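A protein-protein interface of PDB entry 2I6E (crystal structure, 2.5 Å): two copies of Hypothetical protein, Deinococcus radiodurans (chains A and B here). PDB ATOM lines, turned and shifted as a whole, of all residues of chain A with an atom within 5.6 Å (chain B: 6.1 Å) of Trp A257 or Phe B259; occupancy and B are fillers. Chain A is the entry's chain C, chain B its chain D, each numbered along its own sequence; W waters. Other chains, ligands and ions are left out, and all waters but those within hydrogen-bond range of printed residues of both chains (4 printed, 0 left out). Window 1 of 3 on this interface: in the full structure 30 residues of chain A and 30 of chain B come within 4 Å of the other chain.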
ATOM      1  N   LEU A 234     -33.189   8.536  23.351  1.00  0.00           N
ATOM      2  CA  LEU A 234     -32.436   9.786  23.388  1.00  0.00           C
ATOM      3  C   LEU A 234     -33.064  10.909  22.576  1.00  0.00           C
ATOM      4  O   LEU A 234     -33.043  12.058  22.999  1.00  0.00           O
ATOM      5  CB  LEU A 234     -30.991   9.568  22.923  1.00  0.00           C
ATOM      6  CG  LEU A 234     -29.879   9.396  23.973  1.00  0.00           C
ATOM      7  CD1 LEU A 234     -30.413   9.585  25.377  1.00  0.00           C
ATOM      8  CD2 LEU A 234     -29.256   8.016  23.823  1.00  0.00           C
ATOM      9  N   VAL A 252     -28.173  18.459  20.959  1.00  0.00           N
ATOM     10  CA  VAL A 252     -28.490  17.925  22.268  1.00  0.00           C
ATOM     11  C   VAL A 252     -28.416  16.408  22.312  1.00  0.00           C
ATOM     12  O   VAL A 252     -28.018  15.830  23.325  1.00  0.00           O
ATOM     13  CB  VAL A 252     -29.880  18.410  22.734  1.00  0.00           C
ATOM     14  CG1 VAL A 252     -30.265  17.719  24.038  1.00  0.00           C
ATOM     15  CG2 VAL A 252     -29.847  19.924  22.914  1.00  0.00           C
ATOM     16  N   GLN A 253     -28.788  15.757  21.215  1.00  0.00           N
ATOM     17  CA  GLN A 253     -28.738  14.302  21.186  1.00  0.00           C
ATOM     18  C   GLN A 253     -27.277  13.830  21.286  1.00  0.00           C
ATOM     19  O   GLN A 253     -26.959  12.935  22.073  1.00  0.00           O
ATOM     20  CB  GLN A 253     -29.386  13.763  19.918  1.00  0.00           C
ATOM     21  CG  GLN A 253     -29.425  12.262  19.887  1.00  0.00           C
ATOM     22  CD  GLN A 253     -30.172  11.717  18.693  1.00  0.00           C
ATOM     23  OE1 GLN A 253     -31.358  11.998  18.503  1.00  0.00           O
ATOM     24  NE2 GLN A 253     -29.483  10.924  17.878  1.00  0.00           N
ATOM     25  N   HIS A 254     -26.385  14.437  20.509  1.00  0.00           N
ATOM     26  CA  HIS A 254     -24.993  14.035  20.590  1.00  0.00           C
ATOM     27  C   HIS A 254     -24.393  14.412  21.949  1.00  0.00           C
ATOM     28  O   HIS A 254     -23.555  13.694  22.488  1.00  0.00           O
ATOM     29  CB  HIS A 254     -24.152  14.664  19.480  1.00  0.00           C
ATOM     30  CG  HIS A 254     -22.752  14.140  19.444  1.00  0.00           C
ATOM     31  ND1 HIS A 254     -22.462  12.821  19.158  1.00  0.00           N
ATOM     32  CD2 HIS A 254     -21.569  14.725  19.746  1.00  0.00           C
ATOM     33  CE1 HIS A 254     -21.166  12.617  19.291  1.00  0.00           C
ATOM     34  NE2 HIS A 254     -20.600  13.756  19.648  1.00  0.00           N
ATOM     35  N   TYR A 255     -24.817  15.540  22.501  1.00  0.00           N
ATOM     36  CA  TYR A 255     -24.317  15.957  23.801  1.00  0.00           C
ATOM     37  C   TYR A 255     -24.630  14.870  24.849  1.00  0.00           C
ATOM     38  O   TYR A 255     -23.780  14.520  25.666  1.00  0.00           O
ATOM     39  CB  TYR A 255     -24.966  17.284  24.193  1.00  0.00           C
ATOM     40  CG  TYR A 255     -24.672  17.754  25.601  1.00  0.00           C
ATOM     41  CD1 TYR A 255     -23.423  18.262  25.948  1.00  0.00           C
ATOM     42  CD2 TYR A 255     -25.664  17.738  26.575  1.00  0.00           C
ATOM     43  CE1 TYR A 255     -23.173  18.752  27.226  1.00  0.00           C
ATOM     44  CE2 TYR A 255     -25.432  18.220  27.853  1.00  0.00           C
ATOM     45  CZ  TYR A 255     -24.184  18.730  28.180  1.00  0.00           C
ATOM     46  OH  TYR A 255     -23.957  19.219  29.463  1.00  0.00           O
ATOM     47  N   LEU A 256     -25.847  14.338  24.813  1.00  0.00           N
ATOM     48  CA  LEU A 256     -26.267  13.302  25.757  1.00  0.00           C
ATOM     49  C   LEU A 256     -25.612  11.953  25.478  1.00  0.00           C
ATOM     50  O   LEU A 256     -25.164  11.265  26.390  1.00  0.00           O
ATOM     51  CB  LEU A 256     -27.793  13.149  25.730  1.00  0.00           C
ATOM     52  CG  LEU A 256     -28.551  14.404  26.180  1.00  0.00           C
ATOM     53  CD1 LEU A 256     -30.040  14.109  26.237  1.00  0.00           C
ATOM     54  CD2 LEU A 256     -28.037  14.864  27.551  1.00  0.00           C
ATOM     55  N   TRP A 257     -25.575  11.575  24.210  1.00  0.00           N
ATOM     56  CA  TRP A 257     -24.968  10.317  23.805  1.00  0.00           C
ATOM     57  C   TRP A 257     -23.506  10.278  24.253  1.00  0.00           C
ATOM     58  O   TRP A 257     -22.947   9.224  24.562  1.00  0.00           O
ATOM     59  CB  TRP A 257     -25.050  10.190  22.281  1.00  0.00           C
ATOM     60  CG  TRP A 257     -24.117   9.190  21.705  1.00  0.00           C
ATOM     61  CD1 TRP A 257     -22.903   9.435  21.118  1.00  0.00           C
ATOM     62  CD2 TRP A 257     -24.297   7.776  21.686  1.00  0.00           C
ATOM     63  NE1 TRP A 257     -22.321   8.254  20.735  1.00  0.00           N
ATOM     64  CE2 TRP A 257     -23.153   7.219  21.071  1.00  0.00           C
ATOM     65  CE3 TRP A 257     -25.318   6.920  22.130  1.00  0.00           C
ATOM     66  CZ2 TRP A 257     -22.996   5.847  20.887  1.00  0.00           C
ATOM     67  CZ3 TRP A 257     -25.164   5.551  21.947  1.00  0.00           C
ATOM     68  CH2 TRP A 257     -24.007   5.028  21.329  1.00  0.00           C
ATOM     69  N   ASN A 258     -22.901  11.450  24.301  1.00  0.00           N
ATOM     70  CA  ASN A 258     -21.510  11.574  24.665  1.00  0.00           C
ATOM     71  C   ASN A 258     -21.177  11.397  26.154  1.00  0.00           C
ATOM     72  O   ASN A 258     -20.003  11.352  26.513  1.00  0.00           O
ATOM     73  CB  ASN A 258     -21.001  12.916  24.141  1.00  0.00           C
ATOM     74  CG  ASN A 258     -19.529  13.096  24.348  1.00  0.00           C
ATOM     75  OD1 ASN A 258     -19.107  13.809  25.256  1.00  0.00           O
ATOM     76  ND2 ASN A 258     -18.725  12.437  23.515  1.00  0.00           N
ATOM     77  N   PHE A 259     -22.188  11.280  27.018  1.00  0.00           N
ATOM     78  CA  PHE A 259     -21.932  11.104  28.455  1.00  0.00           C
ATOM     79  C   PHE A 259     -21.821   9.651  28.908  1.00  0.00           C
ATOM     80  O   PHE A 259     -22.487   8.755  28.373  1.00  0.00           O
ATOM     81  CB  PHE A 259     -23.012  11.806  29.298  1.00  0.00           C
ATOM     82  CG  PHE A 259     -22.819  13.292  29.409  1.00  0.00           C
ATOM     83  CD1 PHE A 259     -21.802  13.814  30.197  1.00  0.00           C
ATOM     84  CD2 PHE A 259     -23.602  14.168  28.657  1.00  0.00           C
ATOM     85  CE1 PHE A 259     -21.557  15.188  30.232  1.00  0.00           C
ATOM     86  CE2 PHE A 259     -23.364  15.552  28.683  1.00  0.00           C
ATOM     87  CZ  PHE A 259     -22.336  16.062  29.473  1.00  0.00           C
ATOM     88  N   THR B  25     -25.099  -7.234  14.907  1.00  0.00           N
ATOM     89  CA  THR B  25     -25.722  -6.314  15.846  1.00  0.00           C
ATOM     90  C   THR B  25     -25.005  -5.011  16.198  1.00  0.00           C
ATOM     91  O   THR B  25     -25.651  -3.961  16.255  1.00  0.00           O
ATOM     92  CB  THR B  25     -26.071  -7.029  17.163  1.00  0.00           C
ATOM     93  OG1 THR B  25     -26.994  -8.091  16.898  1.00  0.00           O
ATOM     94  CG2 THR B  25     -26.705  -6.060  18.138  1.00  0.00           C
ATOM     95  N   ASN B  26     -23.693  -5.050  16.428  1.00  0.00           N
ATOM     96  CA  ASN B  26     -22.998  -3.823  16.822  1.00  0.00           C
ATOM     97  C   ASN B  26     -23.035  -2.653  15.843  1.00  0.00           C
ATOM     98  O   ASN B  26     -22.695  -1.533  16.217  1.00  0.00           O
ATOM     99  CB  ASN B  26     -21.541  -4.095  17.249  1.00  0.00           C
ATOM    100  CG  ASN B  26     -20.732  -4.852  16.208  1.00  0.00           C
ATOM    101  OD1 ASN B  26     -20.859  -4.624  15.005  1.00  0.00           O
ATOM    102  ND2 ASN B  26     -19.869  -5.748  16.678  1.00  0.00           N
ATOM    103  N   VAL B  84     -16.270   1.284  15.215  1.00  0.00           N
ATOM    104  CA  VAL B  84     -16.918   0.369  16.133  1.00  0.00           C
ATOM    105  C   VAL B  84     -15.824   0.208  17.170  1.00  0.00           C
ATOM    106  O   VAL B  84     -14.840  -0.516  16.947  1.00  0.00           O
ATOM    107  CB  VAL B  84     -17.257  -0.992  15.503  1.00  0.00           C
ATOM    108  CG1 VAL B  84     -17.948  -1.861  16.529  1.00  0.00           C
ATOM    109  CG2 VAL B  84     -18.168  -0.796  14.304  1.00  0.00           C
ATOM    110  N   ALA B  85     -15.987   0.926  18.279  1.00  0.00           N
ATOM    111  CA  ALA B  85     -15.010   0.924  19.355  1.00  0.00           C
ATOM    112  C   ALA B  85     -15.675   0.997  20.714  1.00  0.00           C
ATOM    113  O   ALA B  85     -16.867   1.273  20.817  1.00  0.00           O
ATOM    114  CB  ALA B  85     -14.060   2.112  19.184  1.00  0.00           C
ATOM    115  N   VAL B  86     -14.882   0.758  21.754  1.00  0.00           N
ATOM    116  CA  VAL B  86     -15.356   0.795  23.125  1.00  0.00           C
ATOM    117  C   VAL B  86     -14.230   1.151  24.090  1.00  0.00           C
ATOM    118  O   VAL B  86     -13.048   1.145  23.730  1.00  0.00           O
ATOM    119  CB  VAL B  86     -15.896  -0.570  23.578  1.00  0.00           C
ATOM    120  CG1 VAL B  86     -17.059  -0.983  22.717  1.00  0.00           C
ATOM    121  CG2 VAL B  86     -14.791  -1.599  23.515  1.00  0.00           C
ATOM    122  N   VAL B  90     -16.336  -5.156  25.701  1.00  0.00           N
ATOM    123  CA  VAL B  90     -17.050  -5.039  24.445  1.00  0.00           C
ATOM    124  C   VAL B  90     -18.128  -6.123  24.425  1.00  0.00           C
ATOM    125  O   VAL B  90     -19.018  -6.117  23.580  1.00  0.00           O
ATOM    126  CB  VAL B  90     -16.084  -5.201  23.250  1.00  0.00           C
ATOM    127  CG1 VAL B  90     -15.349  -6.537  23.335  1.00  0.00           C
ATOM    128  CG2 VAL B  90     -16.850  -5.071  21.944  1.00  0.00           C
ATOM    129  N   SER B  92     -18.552  -8.843  23.220  1.00  0.00           N
ATOM    130  CA  SER B  92     -18.653  -9.757  22.088  1.00  0.00           C
ATOM    131  C   SER B  92     -17.305 -10.208  21.500  1.00  0.00           C
ATOM    132  O   SER B  92     -17.237 -10.650  20.347  1.00  0.00           O
ATOM    133  CB  SER B  92     -19.553  -9.159  20.988  1.00  0.00           C
ATOM    134  OG  SER B  92     -19.067  -7.921  20.488  1.00  0.00           O
ATOM    135  N   PHE B 204     -12.410  -1.739  17.066  1.00  0.00           N
ATOM    136  CA  PHE B 204     -12.526  -3.036  16.419  1.00  0.00           C
ATOM    137  C   PHE B 204     -12.779  -2.984  14.928  1.00  0.00           C
ATOM    138  O   PHE B 204     -12.518  -3.962  14.219  1.00  0.00           O
ATOM    139  CB  PHE B 204     -13.631  -3.838  17.085  1.00  0.00           C
ATOM    140  CG  PHE B 204     -13.249  -4.385  18.422  1.00  0.00           C
ATOM    141  CD1 PHE B 204     -12.374  -5.466  18.518  1.00  0.00           C
ATOM    142  CD2 PHE B 204     -13.754  -3.825  19.584  1.00  0.00           C
ATOM    143  CE1 PHE B 204     -12.012  -5.981  19.766  1.00  0.00           C
ATOM    144  CE2 PHE B 204     -13.402  -4.324  20.827  1.00  0.00           C
ATOM    145  CZ  PHE B 204     -12.529  -5.406  20.924  1.00  0.00           C
ATOM    146  N   ILE B 231     -29.013   6.016  17.100  1.00  0.00           N
ATOM    147  CA  ILE B 231     -28.629   6.459  18.436  1.00  0.00           C
ATOM    148  C   ILE B 231     -29.815   7.103  19.165  1.00  0.00           C
ATOM    149  O   ILE B 231     -29.942   6.990  20.391  1.00  0.00           O
ATOM    150  CB  ILE B 231     -27.441   7.453  18.362  1.00  0.00           C
ATOM    151  CG1 ILE B 231     -26.136   6.669  18.156  1.00  0.00           C
ATOM    152  CG2 ILE B 231     -27.385   8.320  19.615  1.00  0.00           C
ATOM    153  CD1 ILE B 231     -24.896   7.543  17.958  1.00  0.00           C
ATOM    154  N   LEU B 234     -32.404   3.805  20.493  1.00  0.00           N
ATOM    155  CA  LEU B 234     -31.751   2.558  20.869  1.00  0.00           C
ATOM    156  C   LEU B 234     -32.718   1.457  21.290  1.00  0.00           C
ATOM    157  O   LEU B 234     -32.540   0.304  20.906  1.00  0.00           O
ATOM    158  CB  LEU B 234     -30.749   2.812  21.994  1.00  0.00           C
ATOM    159  CG  LEU B 234     -29.272   2.972  21.630  1.00  0.00           C
ATOM    160  CD1 LEU B 234     -29.104   3.885  20.440  1.00  0.00           C
ATOM    161  CD2 LEU B 234     -28.533   3.530  22.834  1.00  0.00           C
ATOM    162  N   HIS B 254     -27.772  -2.112  26.411  1.00  0.00           N
ATOM    163  CA  HIS B 254     -26.563  -1.610  27.038  1.00  0.00           C
ATOM    164  C   HIS B 254     -25.415  -1.877  26.075  1.00  0.00           C
ATOM    165  O   HIS B 254     -24.546  -1.026  25.873  1.00  0.00           O
ATOM    166  CB  HIS B 254     -26.255  -2.277  28.372  1.00  0.00           C
ATOM    167  CG  HIS B 254     -25.073  -1.662  29.054  1.00  0.00           C
ATOM    168  ND1 HIS B 254     -25.036  -0.326  29.399  1.00  0.00           N
ATOM    169  CD2 HIS B 254     -23.847  -2.161  29.343  1.00  0.00           C
ATOM    170  CE1 HIS B 254     -23.836  -0.030  29.865  1.00  0.00           C
ATOM    171  NE2 HIS B 254     -23.095  -1.123  29.841  1.00  0.00           N
ATOM    172  N   TYR B 255     -25.435  -3.063  25.472  1.00  0.00           N
ATOM    173  CA  TYR B 255     -24.424  -3.459  24.507  1.00  0.00           C
ATOM    174  C   TYR B 255     -24.251  -2.355  23.447  1.00  0.00           C
ATOM    175  O   TYR B 255     -23.136  -1.908  23.189  1.00  0.00           O
ATOM    176  CB  TYR B 255     -24.839  -4.789  23.857  1.00  0.00           C
ATOM    177  CG  TYR B 255     -23.900  -5.321  22.786  1.00  0.00           C
ATOM    178  CD1 TYR B 255     -22.614  -5.767  23.100  1.00  0.00           C
ATOM    179  CD2 TYR B 255     -24.310  -5.383  21.454  1.00  0.00           C
ATOM    180  CE1 TYR B 255     -21.755  -6.258  22.106  1.00  0.00           C
ATOM    181  CE2 TYR B 255     -23.466  -5.872  20.452  1.00  0.00           C
ATOM    182  CZ  TYR B 255     -22.190  -6.303  20.777  1.00  0.00           C
ATOM    183  OH  TYR B 255     -21.348  -6.732  19.764  1.00  0.00           O
ATOM    184  N   LEU B 256     -25.351  -1.892  22.858  1.00  0.00           N
ATOM    185  CA  LEU B 256     -25.257  -0.851  21.831  1.00  0.00           C
ATOM    186  C   LEU B 256     -24.873   0.509  22.398  1.00  0.00           C
ATOM    187  O   LEU B 256     -24.103   1.250  21.801  1.00  0.00           O
ATOM    188  CB  LEU B 256     -26.576  -0.735  21.063  1.00  0.00           C
ATOM    189  CG  LEU B 256     -26.992  -1.969  20.257  1.00  0.00           C
ATOM    190  CD1 LEU B 256     -28.262  -1.636  19.494  1.00  0.00           C
ATOM    191  CD2 LEU B 256     -25.886  -2.388  19.294  1.00  0.00           C
ATOM    192  N   TRP B 257     -25.421   0.833  23.559  1.00  0.00           N
ATOM    193  CA  TRP B 257     -25.118   2.091  24.206  1.00  0.00           C
ATOM    194  C   TRP B 257     -23.621   2.183  24.495  1.00  0.00           C
ATOM    195  O   TRP B 257     -23.028   3.252  24.459  1.00  0.00           O
ATOM    196  CB  TRP B 257     -25.910   2.192  25.512  1.00  0.00           C
ATOM    197  CG  TRP B 257     -25.402   3.253  26.410  1.00  0.00           C
ATOM    198  CD1 TRP B 257     -24.536   3.099  27.451  1.00  0.00           C
ATOM    199  CD2 TRP B 257     -25.636   4.657  26.283  1.00  0.00           C
ATOM    200  NE1 TRP B 257     -24.209   4.325  27.977  1.00  0.00           N
ATOM    201  CE2 TRP B 257     -24.868   5.299  27.277  1.00  0.00           C
ATOM    202  CE3 TRP B 257     -26.416   5.435  25.424  1.00  0.00           C
ATOM    203  CZ2 TRP B 257     -24.854   6.683  27.432  1.00  0.00           C
ATOM    204  CZ3 TRP B 257     -26.401   6.816  25.581  1.00  0.00           C
ATOM    205  CH2 TRP B 257     -25.624   7.425  26.577  1.00  0.00           C
ATOM    206  N   ASN B 258     -23.018   1.035  24.764  1.00  0.00           N
ATOM    207  CA  ASN B 258     -21.611   0.969  25.104  1.00  0.00           C
ATOM    208  C   ASN B 258     -20.640   1.201  23.944  1.00  0.00           C
ATOM    209  O   ASN B 258     -19.448   1.412  24.165  1.00  0.00           O
ATOM    210  CB  ASN B 258     -21.345  -0.376  25.790  1.00  0.00           C
ATOM    211  CG  ASN B 258     -19.962  -0.466  26.388  1.00  0.00           C
ATOM    212  OD1 ASN B 258     -19.048  -1.031  25.780  1.00  0.00           O
ATOM    213  ND2 ASN B 258     -19.791   0.092  27.579  1.00  0.00           N
ATOM    214  N   PHE B 259     -21.134   1.182  22.713  1.00  0.00           N
ATOM    215  CA  PHE B 259     -20.254   1.393  21.569  1.00  0.00           C
ATOM    216  C   PHE B 259     -19.962   2.854  21.268  1.00  0.00           C
ATOM    217  O   PHE B 259     -20.823   3.720  21.435  1.00  0.00           O
ATOM    218  CB  PHE B 259     -20.818   0.719  20.314  1.00  0.00           C
ATOM    219  CG  PHE B 259     -20.513  -0.751  20.232  1.00  0.00           C
ATOM    220  CD1 PHE B 259     -19.216  -1.190  19.972  1.00  0.00           C
ATOM    221  CD2 PHE B 259     -21.500  -1.695  20.467  1.00  0.00           C
ATOM    222  CE1 PHE B 259     -18.905  -2.557  19.953  1.00  0.00           C
ATOM    223  CE2 PHE B 259     -21.202  -3.064  20.452  1.00  0.00           C
ATOM    224  CZ  PHE B 259     -19.899  -3.495  20.192  1.00  0.00           C
ATOM    225  N   ARG B 260     -18.725   3.112  20.847  1.00  0.00           N
ATOM    226  CA  ARG B 260     -18.274   4.447  20.478  1.00  0.00           C
ATOM    227  C   ARG B 260     -18.201   4.383  18.953  1.00  0.00           C
ATOM    228  O   ARG B 260     -17.402   3.624  18.378  1.00  0.00           O
ATOM    229  CB  ARG B 260     -16.907   4.732  21.104  1.00  0.00           C
ATOM    230  CG  ARG B 260     -16.943   4.918  22.631  1.00  0.00           C
ATOM    231  CD  ARG B 260     -15.532   5.015  23.215  1.00  0.00           C
ATOM    232  NE  ARG B 260     -14.767   6.082  22.577  1.00  0.00           N
ATOM    233  CZ  ARG B 260     -14.985   7.377  22.780  1.00  0.00           C
ATOM    234  NH1 ARG B 260     -15.943   7.759  23.622  1.00  0.00           N
ATOM    235  NH2 ARG B 260     -14.270   8.287  22.121  1.00  0.00           N
ATOM    236  N   TYR B 261     -19.038   5.189  18.304  1.00  0.00           N
ATOM    237  CA  TYR B 261     -19.155   5.174  16.851  1.00  0.00           C
ATOM    238  C   TYR B 261     -18.532   6.283  16.017  1.00  0.00           C
ATOM    239  O   TYR B 261     -18.538   6.196  14.783  1.00  0.00           O
ATOM    240  CB  TYR B 261     -20.636   5.111  16.481  1.00  0.00           C
ATOM    241  CG  TYR B 261     -21.368   3.872  16.923  1.00  0.00           C
ATOM    242  CD1 TYR B 261     -21.060   2.624  16.383  1.00  0.00           C
ATOM    243  CD2 TYR B 261     -22.424   3.954  17.830  1.00  0.00           C
ATOM    244  CE1 TYR B 261     -21.794   1.481  16.735  1.00  0.00           C
ATOM    245  CE2 TYR B 261     -23.165   2.820  18.188  1.00  0.00           C
ATOM    246  CZ  TYR B 261     -22.844   1.591  17.631  1.00  0.00           C
ATOM    247  OH  TYR B 261     -23.590   0.482  17.952  1.00  0.00           O
ATOM    248  N   HIS B 262     -17.985   7.309  16.655  1.00  0.00           N
ATOM    249  CA  HIS B 262     -17.457   8.439  15.900  1.00  0.00           C
ATOM    250  C   HIS B 262     -15.967   8.528  15.581  1.00  0.00           C
ATOM    251  O   HIS B 262     -15.497   9.562  15.080  1.00  0.00           O
ATOM    252  CB  HIS B 262     -17.918   9.728  16.579  1.00  0.00           C
ATOM    253  CG  HIS B 262     -19.399   9.920  16.548  1.00  0.00           C
ATOM    254  ND1 HIS B 262     -20.265   9.146  17.289  1.00  0.00           N
ATOM    255  CD2 HIS B 262     -20.170  10.779  15.841  1.00  0.00           C
ATOM    256  CE1 HIS B 262     -21.507   9.523  17.044  1.00  0.00           C
ATOM    257  NE2 HIS B 262     -21.477  10.513  16.168  1.00  0.00           N
HETATM  258  O   HOH W   1     -16.796  10.291  23.145  1.00  0.00           O
HETATM  259  O   HOH W   2     -31.738   6.228  22.459  1.00  0.00           O
HETATM  260  O   HOH W   3     -23.021   6.326  24.452  1.00  0.00           O
HETATM  261  O   HOH W   4     -19.957   7.455  19.228  1.00  0.00           O
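The side-chain hydroxyl (OH) of Tyr B261 is in hydrogen-bond range of the backbone carbonyl oxygen (O) of Asn B26 (2.8 Å).
CD2 of Leu A234 touches CZ3 of Trp B257, at 3.6 Å.
Ile B231 touches Gln A253 (CG2 to NE2, 3.8 Å).
His B262 touches His A254 (NE2 to CE1, 3.8 Å).
Trp B257 touches Leu A256.
CE3 of Trp A257 touches CG2 of Ile B231, at 3.5 Å.
CH2 of Trp A257 touches O of Leu B256, 3.8 Å away.
Trp A257 touches Phe B259 (CZ2 to O, 3.1 Å).
Trp A257 touches Tyr B261 (CZ2 to CD2, 3.6 Å).
Trp A257 touches His B262.
Phe A259 touches Trp B257 (O to CZ2, 3.3 Å).
Of the printed residues of chain B, Trp A257 touches Ile B231 (3.5 Å), Leu B256 (3.8 Å), Trp B257 (3.6 Å), Phe B259 (3.1 Å), Tyr B261 (3.6 Å) and His B262 (3.99 Å).
Phe B259 touches one residue of chain A.
Printed residues of chain A within 4 Å of His B262: His A254 (3.8 Å) and Trp A257 (3.99 Å).
Printed residues of chain B within 4 Å of Leu A256: Trp B257 (3.9 Å).
Of the printed residues of chain A, Ile B231 touches Leu A234, Gln A253 and Trp A257.
Of the printed residues of chain B, Gln A253 touches Ile B231 (3.8 Å).
Asn B258 touches none of the printed residues of chain A.
His B254 touches none of the printed residues of chain A.
The nearest printed residue of chain A that does not touch Tyr B261 is His A254 (7.6 Å).
Of the 19 printed residues of chain B, 6 touch a printed residue of chain A.
Of the 9 printed residues of chain A, 6 touch a printed residue of chain B.
Hydrophobic or aromatic side chains of chain A within 4 Å of the printed part of chain B: Leu A234, His A254 and Trp A257.
Leu A234 touches Trp B257, but with the chains exchanged Trp A257 does not touch Leu B234 (4.03 Å).
Leu A256 touches Trp B257, and with the chains exchanged Trp A257 touches Leu B256.
Trp B257 touches its own counterpart, Trp A257.
Trp A257 touches Phe B259, and with the chains exchanged Phe A259 touches Trp B257.
Positions printed for both chains: 234, 254, 255, 256, 257, 258 and 259.
Water W4 lies within hydrogen-bond range of a ring nitrogen (ND1) of His B262 (2.6 Å), the backbone NH of Tyr B261 (2.6 Å) and the indole nitrogen of Trp A257 (2.9 Å).
Water W1 lies within hydrogen-bond range of the guanidinium group of Arg B260 (2.7 Å) and the side-chain amide nitrogen of Asn A258 (2.9 Å).
Water W2 lies within hydrogen-bond range of the backbone carbonyl oxygen of Ile B231 (2.8 Å), the backbone NH of Leu A234 (2.9 Å) and the backbone NH of Leu B234 (3.2 Å).
Water W3 bridges the backbone carbonyl oxygen (O) of Trp A257 and the backbone carbonyl oxygen (O) of Trp B257.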
